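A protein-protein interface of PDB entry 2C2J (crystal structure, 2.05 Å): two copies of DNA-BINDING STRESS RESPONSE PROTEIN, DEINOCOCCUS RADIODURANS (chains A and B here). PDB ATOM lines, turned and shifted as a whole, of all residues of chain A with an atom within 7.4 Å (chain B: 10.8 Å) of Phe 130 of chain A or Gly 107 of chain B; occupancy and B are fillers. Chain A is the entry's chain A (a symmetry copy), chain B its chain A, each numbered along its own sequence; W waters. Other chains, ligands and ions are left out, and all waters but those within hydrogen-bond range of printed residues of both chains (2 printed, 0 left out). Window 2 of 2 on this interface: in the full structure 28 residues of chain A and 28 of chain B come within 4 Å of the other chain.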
ATOM      1  N   GLN A  68      -2.731  -0.408  22.226  1.00  0.00           N
ATOM      2  CA  GLN A  68      -2.161   0.601  21.323  1.00  0.00           C
ATOM      3  C   GLN A  68      -0.871   0.103  20.668  1.00  0.00           C
ATOM      4  O   GLN A  68      -0.689   0.184  19.452  1.00  0.00           O
ATOM      5  CB  GLN A  68      -1.860   1.878  22.136  1.00  0.00           C
ATOM      6  CG  GLN A  68      -1.158   2.949  21.349  1.00  0.00           C
ATOM      7  CD  GLN A  68      -2.120   3.670  20.459  1.00  0.00           C
ATOM      8  OE1 GLN A  68      -3.342   3.429  20.522  1.00  0.00           O
ATOM      9  NE2 GLN A  68      -1.600   4.559  19.615  1.00  0.00           N
ATOM     10  N   TRP A  71      -1.407  -2.641  17.981  1.00  0.00           N
ATOM     11  CA  TRP A  71      -1.769  -2.159  16.630  1.00  0.00           C
ATOM     12  C   TRP A  71      -0.641  -1.421  15.920  1.00  0.00           C
ATOM     13  O   TRP A  71      -0.473  -1.563  14.715  1.00  0.00           O
ATOM     14  CB  TRP A  71      -3.042  -1.260  16.654  1.00  0.00           C
ATOM     15  CG  TRP A  71      -4.287  -2.014  17.065  1.00  0.00           C
ATOM     16  CD1 TRP A  71      -5.103  -1.734  18.126  1.00  0.00           C
ATOM     17  CD2 TRP A  71      -4.830  -3.185  16.437  1.00  0.00           C
ATOM     18  NE1 TRP A  71      -6.116  -2.662  18.196  1.00  0.00           N
ATOM     19  CE2 TRP A  71      -5.970  -3.567  17.177  1.00  0.00           C
ATOM     20  CE3 TRP A  71      -4.448  -3.966  15.324  1.00  0.00           C
ATOM     21  CZ2 TRP A  71      -6.761  -4.707  16.840  1.00  0.00           C
ATOM     22  CZ3 TRP A  71      -5.234  -5.112  14.985  1.00  0.00           C
ATOM     23  CH2 TRP A  71      -6.378  -5.457  15.751  1.00  0.00           C
ATOM     24  N   ASN A  72       0.127  -0.646  16.679  1.00  0.00           N
ATOM     25  CA  ASN A  72       1.068   0.340  16.107  1.00  0.00           C
ATOM     26  C   ASN A  72       2.529  -0.081  16.020  1.00  0.00           C
ATOM     27  O   ASN A  72       3.329   0.597  15.344  1.00  0.00           O
ATOM     28  CB  ASN A  72       0.881   1.710  16.785  1.00  0.00           C
ATOM     29  CG  ASN A  72      -0.500   2.286  16.489  1.00  0.00           C
ATOM     30  OD1 ASN A  72      -0.773   2.642  15.368  1.00  0.00           O
ATOM     31  ND2 ASN A  72      -1.402   2.267  17.459  1.00  0.00           N
ATOM     32  N   VAL A  73       2.860  -1.233  16.617  1.00  0.00           N
ATOM     33  CA  VAL A  73       4.249  -1.670  16.677  1.00  0.00           C
ATOM     34  C   VAL A  73       4.733  -2.003  15.252  1.00  0.00           C
ATOM     35  O   VAL A  73       3.920  -2.402  14.414  1.00  0.00           O
ATOM     36  CB  VAL A  73       4.464  -2.814  17.704  1.00  0.00           C
ATOM     37  CG1 VAL A  73       3.671  -4.124  17.316  1.00  0.00           C
ATOM     38  CG2 VAL A  73       5.972  -3.092  17.919  1.00  0.00           C
ATOM     39  N   SER A  74       6.032  -1.792  14.991  1.00  0.00           N
ATOM     40  CA  SER A  74       6.618  -1.770  13.622  1.00  0.00           C
ATOM     41  C   SER A  74       8.053  -2.312  13.736  1.00  0.00           C
ATOM     42  O   SER A  74       8.629  -2.233  14.783  1.00  0.00           O
ATOM     43  CB  SER A  74       6.681  -0.323  13.086  1.00  0.00           C
ATOM     44  OG  SER A  74       5.416   0.301  13.158  1.00  0.00           O
ATOM     45  N   PRO A 127       3.545   6.870  23.699  1.00  0.00           N
ATOM     46  CA  PRO A 127       3.464   7.799  22.553  1.00  0.00           C
ATOM     47  C   PRO A 127       2.443   7.344  21.503  1.00  0.00           C
ATOM     48  O   PRO A 127       2.183   6.129  21.371  1.00  0.00           O
ATOM     49  CB  PRO A 127       4.869   7.742  21.932  1.00  0.00           C
ATOM     50  CG  PRO A 127       5.735   6.993  22.910  1.00  0.00           C
ATOM     51  CD  PRO A 127       4.863   6.217  23.820  1.00  0.00           C
ATOM     52  N   GLY A 128       1.864   8.312  20.794  1.00  0.00           N
ATOM     53  CA  GLY A 128       1.001   8.043  19.652  1.00  0.00           C
ATOM     54  C   GLY A 128       1.861   7.757  18.443  1.00  0.00           C
ATOM     55  O   GLY A 128       3.091   7.866  18.510  1.00  0.00           O
ATOM     56  N   GLY A 129       1.224   7.383  17.338  1.00  0.00           N
ATOM     57  CA  GLY A 129       1.953   7.176  16.095  1.00  0.00           C
ATOM     58  C   GLY A 129       2.465   5.754  15.971  1.00  0.00           C
ATOM     59  O   GLY A 129       2.256   4.930  16.875  1.00  0.00           O
ATOM     60  N   PHE A 130       3.130   5.464  14.852  1.00  0.00           N
ATOM     61  CA  PHE A 130       3.838   4.202  14.690  1.00  0.00           C
ATOM     62  C   PHE A 130       4.937   4.047  15.751  1.00  0.00           C
ATOM     63  O   PHE A 130       5.700   4.974  15.992  1.00  0.00           O
ATOM     64  CB  PHE A 130       4.391   4.060  13.267  1.00  0.00           C
ATOM     65  CG  PHE A 130       3.338   4.017  12.218  1.00  0.00           C
ATOM     66  CD1 PHE A 130       2.473   2.907  12.110  1.00  0.00           C
ATOM     67  CD2 PHE A 130       3.179   5.089  11.330  1.00  0.00           C
ATOM     68  CE1 PHE A 130       1.494   2.862  11.139  1.00  0.00           C
ATOM     69  CE2 PHE A 130       2.182   5.055  10.350  1.00  0.00           C
ATOM     70  CZ  PHE A 130       1.355   3.925  10.241  1.00  0.00           C
ATOM     71  N   LEU A 131       4.995   2.877  16.389  1.00  0.00           N
ATOM     72  CA  LEU A 131       5.924   2.628  17.484  1.00  0.00           C
ATOM     73  C   LEU A 131       6.928   1.618  17.089  1.00  0.00           C
ATOM     74  O   LEU A 131       6.581   0.587  16.522  1.00  0.00           O
ATOM     75  CB  LEU A 131       5.184   2.111  18.715  1.00  0.00           C
ATOM     76  CG  LEU A 131       4.226   3.033  19.418  1.00  0.00           C
ATOM     77  CD1 LEU A 131       3.562   2.274  20.621  1.00  0.00           C
ATOM     78  CD2 LEU A 131       4.957   4.303  19.898  1.00  0.00           C
ATOM     79  N   ASP A 132       8.241   1.848  17.396  1.00  0.00           N
ATOM     80  CA  ASP A 132       9.257   0.878  17.010  1.00  0.00           C
ATOM     81  C   ASP A 132       9.250  -0.284  17.989  1.00  0.00           C
ATOM     82  O   ASP A 132       8.949  -0.093  19.175  1.00  0.00           O
ATOM     83  CB  ASP A 132      10.645   1.503  16.990  1.00  0.00           C
ATOM     84  CG  ASP A 132      11.672   0.574  16.430  1.00  0.00           C
ATOM     85  OD1 ASP A 132      11.495   0.122  15.283  1.00  0.00           O
ATOM     86  OD2 ASP A 132      12.664   0.255  17.117  1.00  0.00           O
ATOM     87  N   GLN A 135      11.403   0.367  21.106  1.00  0.00           N
ATOM     88  CA  GLN A 135      10.676   1.299  21.972  1.00  0.00           C
ATOM     89  C   GLN A 135       9.523   0.622  22.781  1.00  0.00           C
ATOM     90  O   GLN A 135       9.357   0.864  23.978  1.00  0.00           O
ATOM     91  CB  GLN A 135      10.171   2.433  21.066  1.00  0.00           C
ATOM     92  CG  GLN A 135       9.180   3.400  21.678  1.00  0.00           C
ATOM     93  CD  GLN A 135       8.683   4.439  20.662  1.00  0.00           C
ATOM     94  OE1 GLN A 135       8.609   4.164  19.445  1.00  0.00           O
ATOM     95  NE2 GLN A 135       8.355   5.638  21.152  1.00  0.00           N
ATOM     96  N   VAL A 136       8.735  -0.256  22.137  1.00  0.00           N
ATOM     97  CA  VAL A 136       7.702  -1.046  22.880  1.00  0.00           C
ATOM     98  C   VAL A 136       8.361  -1.883  23.986  1.00  0.00           C
ATOM     99  O   VAL A 136       7.920  -1.901  25.139  1.00  0.00           O
ATOM    100  CB  VAL A 136       6.846  -1.924  21.866  1.00  0.00           C
ATOM    101  CG1 VAL A 136       5.917  -2.945  22.581  1.00  0.00           C
ATOM    102  CG2 VAL A 136       6.032  -0.993  20.958  1.00  0.00           C
ATOM    103  N   THR B  42      -4.576  12.279  -0.939  1.00  0.00           N
ATOM    104  CA  THR B  42      -4.577  12.245   0.556  1.00  0.00           C
ATOM    105  C   THR B  42      -5.766  13.001   1.176  1.00  0.00           C
ATOM    106  O   THR B  42      -5.915  13.031   2.401  1.00  0.00           O
ATOM    107  CB  THR B  42      -3.235  12.770   1.156  1.00  0.00           C
ATOM    108  OG1 THR B  42      -2.744  13.864   0.364  1.00  0.00           O
ATOM    109  CG2 THR B  42      -2.177  11.650   1.213  1.00  0.00           C
ATOM    110  N   ASP B  44      -8.765  12.124   0.264  1.00  0.00           N
ATOM    111  CA  ASP B  44      -9.630  10.968   0.326  1.00  0.00           C
ATOM    112  C   ASP B  44      -9.204  10.101   1.516  1.00  0.00           C
ATOM    113  O   ASP B  44     -10.039   9.713   2.344  1.00  0.00           O
ATOM    114  CB  ASP B  44      -9.515  10.199  -0.991  1.00  0.00           C
ATOM    115  CG  ASP B  44      -9.673  11.109  -2.219  1.00  0.00           C
ATOM    116  OD1 ASP B  44      -8.669  11.760  -2.624  1.00  0.00           O
ATOM    117  OD2 ASP B  44     -10.802  11.172  -2.770  1.00  0.00           O
ATOM    118  N   LEU B  45      -7.902   9.820   1.603  1.00  0.00           N
ATOM    119  CA  LEU B  45      -7.330   9.120   2.748  1.00  0.00           C
ATOM    120  C   LEU B  45      -7.666   9.812   4.081  1.00  0.00           C
ATOM    121  O   LEU B  45      -8.015   9.139   5.056  1.00  0.00           O
ATOM    122  CB  LEU B  45      -5.812   8.947   2.585  1.00  0.00           C
ATOM    123  CG  LEU B  45      -5.057   8.044   3.578  1.00  0.00           C
ATOM    124  CD1 LEU B  45      -3.975   7.225   2.884  1.00  0.00           C
ATOM    125  CD2 LEU B  45      -4.448   8.851   4.714  1.00  0.00           C
ATOM    126  N   LYS B  46      -7.571  11.144   4.115  1.00  0.00           N
ATOM    127  CA  LYS B  46      -7.899  11.926   5.314  1.00  0.00           C
ATOM    128  C   LYS B  46      -9.328  11.663   5.807  1.00  0.00           C
ATOM    129  O   LYS B  46      -9.554  11.520   7.008  1.00  0.00           O
ATOM    130  CB  LYS B  46      -7.695  13.426   5.060  1.00  0.00           C
ATOM    131  CG  LYS B  46      -7.839  14.293   6.306  1.00  0.00           C
ATOM    132  CD  LYS B  46      -7.691  15.790   5.990  1.00  0.00           C
ATOM    133  CE  LYS B  46      -7.689  16.647   7.262  1.00  0.00           C
ATOM    134  NZ  LYS B  46      -8.996  16.577   7.994  1.00  0.00           N
ATOM    135  N   SER B  48     -11.186   8.973   5.358  1.00  0.00           N
ATOM    136  CA  SER B  48     -11.321   7.632   5.888  1.00  0.00           C
ATOM    137  C   SER B  48     -10.734   7.541   7.294  1.00  0.00           C
ATOM    138  O   SER B  48     -11.352   6.989   8.187  1.00  0.00           O
ATOM    139  CB  SER B  48     -10.675   6.630   4.941  1.00  0.00           C
ATOM    140  OG  SER B  48     -11.649   6.187   4.007  1.00  0.00           O
ATOM    141  N   VAL B  49      -9.558   8.124   7.459  1.00  0.00           N
ATOM    142  CA  VAL B  49      -8.809   8.114   8.694  1.00  0.00           C
ATOM    143  C   VAL B  49      -9.581   8.822   9.792  1.00  0.00           C
ATOM    144  O   VAL B  49      -9.641   8.342  10.942  1.00  0.00           O
ATOM    145  CB  VAL B  49      -7.388   8.727   8.475  1.00  0.00           C
ATOM    146  CG1 VAL B  49      -6.641   8.940   9.776  1.00  0.00           C
ATOM    147  CG2 VAL B  49      -6.583   7.806   7.595  1.00  0.00           C
ATOM    148  N   GLN B  50     -10.194   9.944   9.419  1.00  0.00           N
ATOM    149  CA  GLN B  50     -10.976  10.741  10.340  1.00  0.00           C
ATOM    150  C   GLN B  50     -12.214   9.952  10.814  1.00  0.00           C
ATOM    151  O   GLN B  50     -12.503   9.884  12.002  1.00  0.00           O
ATOM    152  CB  GLN B  50     -11.392  12.071   9.657  1.00  0.00           C
ATOM    153  CG  GLN B  50     -12.506  12.866  10.360  1.00  0.00           C
ATOM    154  CD  GLN B  50     -13.016  14.075   9.512  1.00  0.00           C
ATOM    155  OE1 GLN B  50     -13.840  13.916   8.588  1.00  0.00           O
ATOM    156  NE2 GLN B  50     -12.534  15.275   9.842  1.00  0.00           N
ATOM    157  N   LEU B  52     -12.680   6.703  10.732  1.00  0.00           N
ATOM    158  CA  LEU B  52     -12.264   5.514  11.514  1.00  0.00           C
ATOM    159  C   LEU B  52     -11.819   5.899  12.905  1.00  0.00           C
ATOM    160  O   LEU B  52     -12.262   5.305  13.887  1.00  0.00           O
ATOM    161  CB  LEU B  52     -11.133   4.770  10.799  1.00  0.00           C
ATOM    162  CG  LEU B  52     -11.573   3.926   9.613  1.00  0.00           C
ATOM    163  CD1 LEU B  52     -10.342   3.615   8.713  1.00  0.00           C
ATOM    164  CD2 LEU B  52     -12.263   2.635  10.080  1.00  0.00           C
ATOM    165  N   GLN B  53     -10.971   6.928  12.991  1.00  0.00           N
ATOM    166  CA  GLN B  53     -10.452   7.375  14.278  1.00  0.00           C
ATOM    167  C   GLN B  53     -11.584   7.828  15.193  1.00  0.00           C
ATOM    168  O   GLN B  53     -11.625   7.491  16.382  1.00  0.00           O
ATOM    169  CB  GLN B  53      -9.444   8.524  14.092  1.00  0.00           C
ATOM    170  CG  GLN B  53      -8.893   9.057  15.387  1.00  0.00           C
ATOM    171  CD  GLN B  53      -8.153   7.985  16.204  1.00  0.00           C
ATOM    172  OE1 GLN B  53      -7.187   7.378  15.721  1.00  0.00           O
ATOM    173  NE2 GLN B  53      -8.622   7.740  17.432  1.00  0.00           N
ATOM    174  N   VAL B  99     -11.988  -1.723  13.852  1.00  0.00           N
ATOM    175  CA  VAL B  99     -11.744  -0.320  13.472  1.00  0.00           C
ATOM    176  C   VAL B  99     -10.244   0.041  13.473  1.00  0.00           C
ATOM    177  O   VAL B  99      -9.702   0.574  12.475  1.00  0.00           O
ATOM    178  CB  VAL B  99     -12.625   0.658  14.303  1.00  0.00           C
ATOM    179  CG1 VAL B  99     -12.239   2.172  14.025  1.00  0.00           C
ATOM    180  CG2 VAL B  99     -14.125   0.501  13.908  1.00  0.00           C
ATOM    181  N   ALA B 100      -9.555  -0.232  14.575  1.00  0.00           N
ATOM    182  CA  ALA B 100      -8.127   0.005  14.644  1.00  0.00           C
ATOM    183  C   ALA B 100      -7.382  -0.747  13.557  1.00  0.00           C
ATOM    184  O   ALA B 100      -6.517  -0.205  12.901  1.00  0.00           O
ATOM    185  CB  ALA B 100      -7.618  -0.410  16.021  1.00  0.00           C
ATOM    186  N   GLU B 101      -7.716  -2.023  13.373  1.00  0.00           N
ATOM    187  CA  GLU B 101      -7.091  -2.820  12.321  1.00  0.00           C
ATOM    188  C   GLU B 101      -7.336  -2.199  10.944  1.00  0.00           C
ATOM    189  O   GLU B 101      -6.436  -2.161  10.105  1.00  0.00           O
ATOM    190  CB  GLU B 101      -7.657  -4.253  12.383  1.00  0.00           C
ATOM    191  CG  GLU B 101      -7.228  -5.201  11.268  1.00  0.00           C
ATOM    192  CD  GLU B 101      -8.056  -6.486  11.358  1.00  0.00           C
ATOM    193  OE1 GLU B 101      -9.053  -6.661  10.604  1.00  0.00           O
ATOM    194  OE2 GLU B 101      -7.748  -7.265  12.254  1.00  0.00           O
ATOM    195  N   ARG B 102      -8.558  -1.725  10.702  1.00  0.00           N
ATOM    196  CA  ARG B 102      -8.817  -1.045   9.449  1.00  0.00           C
ATOM    197  C   ARG B 102      -7.980   0.234   9.261  1.00  0.00           C
ATOM    198  O   ARG B 102      -7.461   0.498   8.173  1.00  0.00           O
ATOM    199  CB  ARG B 102     -10.321  -0.769   9.259  1.00  0.00           C
ATOM    200  CG  ARG B 102     -10.624  -0.104   7.914  1.00  0.00           C
ATOM    201  CD  ARG B 102     -10.412  -1.052   6.742  1.00  0.00           C
ATOM    202  NE  ARG B 102     -10.686  -0.373   5.464  1.00  0.00           N
ATOM    203  CZ  ARG B 102     -10.143  -0.718   4.299  1.00  0.00           C
ATOM    204  NH1 ARG B 102      -9.312  -1.769   4.209  1.00  0.00           N
ATOM    205  NH2 ARG B 102     -10.427  -0.011   3.210  1.00  0.00           N
ATOM    206  N   GLN B 103      -7.814   1.010  10.328  1.00  0.00           N
ATOM    207  CA  GLN B 103      -6.914   2.149  10.253  1.00  0.00           C
ATOM    208  C   GLN B 103      -5.535   1.736   9.804  1.00  0.00           C
ATOM    209  O   GLN B 103      -4.992   2.322   8.866  1.00  0.00           O
ATOM    210  CB  GLN B 103      -6.789   2.862  11.600  1.00  0.00           C
ATOM    211  CG  GLN B 103      -8.009   3.590  12.012  1.00  0.00           C
ATOM    212  CD  GLN B 103      -7.859   4.105  13.422  1.00  0.00           C
ATOM    213  OE1 GLN B 103      -7.896   3.317  14.387  1.00  0.00           O
ATOM    214  NE2 GLN B 103      -7.612   5.401  13.556  1.00  0.00           N
ATOM    215  N   LEU B 104      -4.967   0.726  10.454  1.00  0.00           N
ATOM    216  CA  LEU B 104      -3.652   0.248  10.028  1.00  0.00           C
ATOM    217  C   LEU B 104      -3.645  -0.240   8.572  1.00  0.00           C
ATOM    218  O   LEU B 104      -2.660  -0.031   7.838  1.00  0.00           O
ATOM    219  CB  LEU B 104      -3.100  -0.827  10.985  1.00  0.00           C
ATOM    220  CG  LEU B 104      -2.255  -0.310  12.172  1.00  0.00           C
ATOM    221  CD1 LEU B 104      -0.932   0.381  11.681  1.00  0.00           C
ATOM    222  CD2 LEU B 104      -3.022   0.611  13.173  1.00  0.00           C
ATOM    223  N   SER B 105      -4.747  -0.864   8.162  1.00  0.00           N
ATOM    224  CA  SER B 105      -4.886  -1.415   6.823  1.00  0.00           C
ATOM    225  C   SER B 105      -4.900  -0.342   5.720  1.00  0.00           C
ATOM    226  O   SER B 105      -4.507  -0.613   4.587  1.00  0.00           O
ATOM    227  CB  SER B 105      -6.130  -2.269   6.734  1.00  0.00           C
ATOM    228  OG  SER B 105      -6.046  -3.375   7.627  1.00  0.00           O
ATOM    229  N   VAL B 106      -5.383   0.851   6.039  1.00  0.00           N
ATOM    230  CA  VAL B 106      -5.351   1.934   5.051  1.00  0.00           C
ATOM    231  C   VAL B 106      -4.067   2.750   5.216  1.00  0.00           C
ATOM    232  O   VAL B 106      -3.857   3.735   4.522  1.00  0.00           O
ATOM    233  CB  VAL B 106      -6.668   2.798   5.033  1.00  0.00           C
ATOM    234  CG1 VAL B 106      -7.864   1.927   4.736  1.00  0.00           C
ATOM    235  CG2 VAL B 106      -6.856   3.570   6.329  1.00  0.00           C
ATOM    236  N   GLY B 107      -3.181   2.300   6.111  1.00  0.00           N
ATOM    237  CA  GLY B 107      -1.849   2.868   6.224  1.00  0.00           C
ATOM    238  C   GLY B 107      -1.694   3.959   7.258  1.00  0.00           C
ATOM    239  O   GLY B 107      -0.689   4.645   7.271  1.00  0.00           O
ATOM    240  N   ALA B 108      -2.646   4.078   8.173  1.00  0.00           N
ATOM    241  CA  ALA B 108      -2.579   5.081   9.238  1.00  0.00           C
ATOM    242  C   ALA B 108      -2.422   4.456  10.630  1.00  0.00           C
ATOM    243  O   ALA B 108      -2.971   3.386  10.923  1.00  0.00           O
ATOM    244  CB  ALA B 108      -3.836   5.927   9.235  1.00  0.00           C
ATOM    245  N   SER B 109      -1.679   5.150  11.472  1.00  0.00           N
ATOM    246  CA  SER B 109      -1.554   4.817  12.884  1.00  0.00           C
ATOM    247  C   SER B 109      -2.914   4.952  13.576  1.00  0.00           C
ATOM    248  O   SER B 109      -3.724   5.791  13.178  1.00  0.00           O
ATOM    249  CB  SER B 109      -0.532   5.739  13.546  1.00  0.00           C
ATOM    250  OG  SER B 109      -0.450   5.396  14.914  1.00  0.00           O
ATOM    251  N   SER B 110      -3.173   4.118  14.595  1.00  0.00           N
ATOM    252  CA  SER B 110      -4.469   4.121  15.287  1.00  0.00           C
ATOM    253  C   SER B 110      -4.283   4.773  16.657  1.00  0.00           C
ATOM    254  O   SER B 110      -3.393   4.380  17.405  1.00  0.00           O
ATOM    255  CB  SER B 110      -4.984   2.654  15.455  1.00  0.00           C
ATOM    256  OG  SER B 110      -6.143   2.599  16.283  1.00  0.00           O
ATOM    257  N   ASP B 111      -5.102   5.760  17.022  1.00  0.00           N
ATOM    258  CA  ASP B 111      -4.891   6.378  18.348  1.00  0.00           C
ATOM    259  C   ASP B 111      -5.952   5.900  19.340  1.00  0.00           C
ATOM    260  O   ASP B 111      -7.069   6.421  19.377  1.00  0.00           O
ATOM    261  CB  ASP B 111      -4.817   7.934  18.294  1.00  0.00           C
ATOM    262  CG  ASP B 111      -4.379   8.541  19.623  1.00  0.00           C
ATOM    263  OD1 ASP B 111      -4.430   7.846  20.652  1.00  0.00           O
ATOM    264  OD2 ASP B 111      -3.992   9.738  19.658  1.00  0.00           O
ATOM    265  N   GLY B 112      -5.566   4.921  20.155  1.00  0.00           N
ATOM    266  CA  GLY B 112      -6.472   4.306  21.111  1.00  0.00           C
ATOM    267  C   GLY B 112      -6.124   4.611  22.546  1.00  0.00           C
ATOM    268  O   GLY B 112      -6.509   3.860  23.455  1.00  0.00           O
ATOM    269  N   ARG B 113      -5.389   5.712  22.762  1.00  0.00           N
ATOM    270  CA  ARG B 113      -4.859   6.036  24.103  1.00  0.00           C
ATOM    271  C   ARG B 113      -5.907   6.648  25.010  1.00  0.00           C
ATOM    272  O   ARG B 113      -6.853   7.275  24.533  1.00  0.00           O
ATOM    273  CB  ARG B 113      -3.641   6.970  24.002  1.00  0.00           C
ATOM    274  CG  ARG B 113      -2.500   6.368  23.189  1.00  0.00           C
ATOM    275  CD  ARG B 113      -1.457   7.395  22.817  1.00  0.00           C
ATOM    276  NE  ARG B 113      -2.002   8.514  22.026  1.00  0.00           N
ATOM    277  CZ  ARG B 113      -1.570   9.763  22.151  1.00  0.00           C
ATOM    278  NH1 ARG B 113      -0.590  10.013  23.004  1.00  0.00           N
ATOM    279  NH2 ARG B 113      -2.076  10.746  21.418  1.00  0.00           N
ATOM    280  N   ASP B 162     -14.108   5.150  -0.190  1.00  0.00           N
ATOM    281  CA  ASP B 162     -13.628   3.978   0.547  1.00  0.00           C
ATOM    282  C   ASP B 162     -14.812   3.111   0.986  1.00  0.00           C
ATOM    283  O   ASP B 162     -15.202   3.120   2.161  1.00  0.00           O
ATOM    284  CB  ASP B 162     -12.758   4.456   1.728  1.00  0.00           C
ATOM    285  CG  ASP B 162     -12.005   3.322   2.438  1.00  0.00           C
ATOM    286  OD1 ASP B 162     -12.235   2.115   2.157  1.00  0.00           O
ATOM    287  OD2 ASP B 162     -11.183   3.654   3.304  1.00  0.00           O
ATOM    288  N   THR B 165     -14.070   0.621   3.931  1.00  0.00           N
ATOM    289  CA  THR B 165     -14.215   1.281   5.215  1.00  0.00           C
ATOM    290  C   THR B 165     -15.695   1.576   5.547  1.00  0.00           C
ATOM    291  O   THR B 165     -16.153   1.315   6.674  1.00  0.00           O
ATOM    292  CB  THR B 165     -13.358   2.515   5.323  1.00  0.00           C
ATOM    293  OG1 THR B 165     -11.966   2.141   5.342  1.00  0.00           O
ATOM    294  CG2 THR B 165     -13.680   3.314   6.586  1.00  0.00           C
HETATM  295  O   HOH W   1      -5.031   1.519  18.745  1.00  0.00           O
HETATM  296  O   HOH W   2      -1.608   6.919  17.318  1.00  0.00           O
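Water W2 lies within hydrogen-bond range of N of Gly 129 of chain A (2.9 Å), OG of Ser 109 of chain B (3.1 Å), O of Ser 110 of chain B (3.1 Å) and NE2 of Gln 68 of chain A (3.3 Å). Water W1 lies within hydrogen-bond range of OG of Ser 110 of chain B (2.9 Å) and OE1 of Gln 68 of chain A (3.1 Å).
NE2 of Gln 53 of chain B sits at hydrogen-bond distance from O of Asp 111 of chain B. O of Glu 101 of chain B sits at hydrogen-bond distance from OG of Ser 105 of chain B (2.8 Å). The side-chain amide oxygen of Gln 103 of chain B is in hydrogen-bond range of the side-chain hydroxyl of Ser 110 of chain B (2.7 Å). The guanidinium group (NH2) of Arg 113 of chain B is in salt-bridge range of the side-chain carboxylate (OD2) of Asp 111 of chain B, at 2.8 Å. The side-chain amide nitrogen (ND2) of Asn 72 of chain A lies within hydrogen-bond range of the backbone carbonyl oxygen (O) of Gln 68 of chain A. The backbone carbonyl oxygen (O) of Asn 72 of chain A sits at hydrogen-bond distance from the backbone NH (N) of Leu 131 of chain A, at 3.0 Å.
Of the printed residues of chain B, Asn 72 of chain A touches Leu 104 (3.7 Å), Ser 109 (2.8 Å) and Ser 110 (2.9 Å). Printed residues of chain B within 4 Å of Gly 129 of chain A: Ser 109 (3.1 Å). Phe 130 of chain A touches just these residues of chain B: Leu 104, Gly 107, Ala 108 and Ser 109. No residue of chain B comes within 4 Å of Leu 131 of chain A. Thr 42 of chain B touches none of the printed residues of chain A. Of the printed residues of chain A, Glu 101 of chain B touches Trp 71. Gly 107 of chain B touches just one residue of chain A: Phe 130 (3.7 Å). Of the printed residues of chain A, Ser 110 of chain B touches Gln 68 and Asn 72. Of the printed residues of chain A, Asp 111 of chain B touches Gln 68. The nearest printed residue of chain A that does not touch Asp 111 of chain B is Asn 72 of chain A (5.1 Å).
No position is printed for both chains.
The side-chain hydroxyl of Ser 109 of chain B lies within hydrogen-bond range of the side-chain amide oxygen of Asn 72 of chain A (2.8 Å). OG of Ser 109 of chain B lies close to O of Gly 129 of chain A (3.4 Å). O of Ser 110 of chain B is in hydrogen-bond range of NE2 of Gln 68 of chain A (2.9 Å). O of Ser 110 of chain B lies within hydrogen-bond range of ND2 of Asn 72 of chain A. The backbone NH (N) of Gly 112 of chain B is in hydrogen-bond range of the side-chain amide oxygen (OE1) of Gln 68 of chain A, at 2.7 Å.
N of Arg 113 of chain B touches OE1 of Gln 68 of chain A, 3.8 Å away. Trp 71 of chain A touches Ala 100 of chain B. CZ3 of Trp 71 of chain A touches CB of Glu 101 of chain B (3.7 Å). O of Trp 71 of chain A touches CG of Leu 104 of chain B, at 3.3 Å. Leu 104 of chain B touches Asn 72 of chain A (CD2 to OD1, 3.7 Å). Gly 128 of chain A touches Arg 113 of chain B. Phe 130 of chain A touches Leu 104 of chain B. Phe 130 of chain A touches Gly 107 of chain B. CZ of Phe 130 of chain A touches C of Ala 108 of chain B, 3.8 Å away. CZ of Phe 130 of chain A touches N of Ser 109 of chain B (3.5 Å).
Printed residues of chain A that touch a printed residue of chain B: Gln 68, Trp 71, Asn 72, Gly 128, Gly 129 and Phe 130. Hydrophobic or aromatic side chains of chain A that line the printed part of chain B: Trp 71 and Phe 130. Hydrophobic or aromatic side chains of chain B within 4 Å of the printed part of chain A: Ala 100 and Leu 104.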
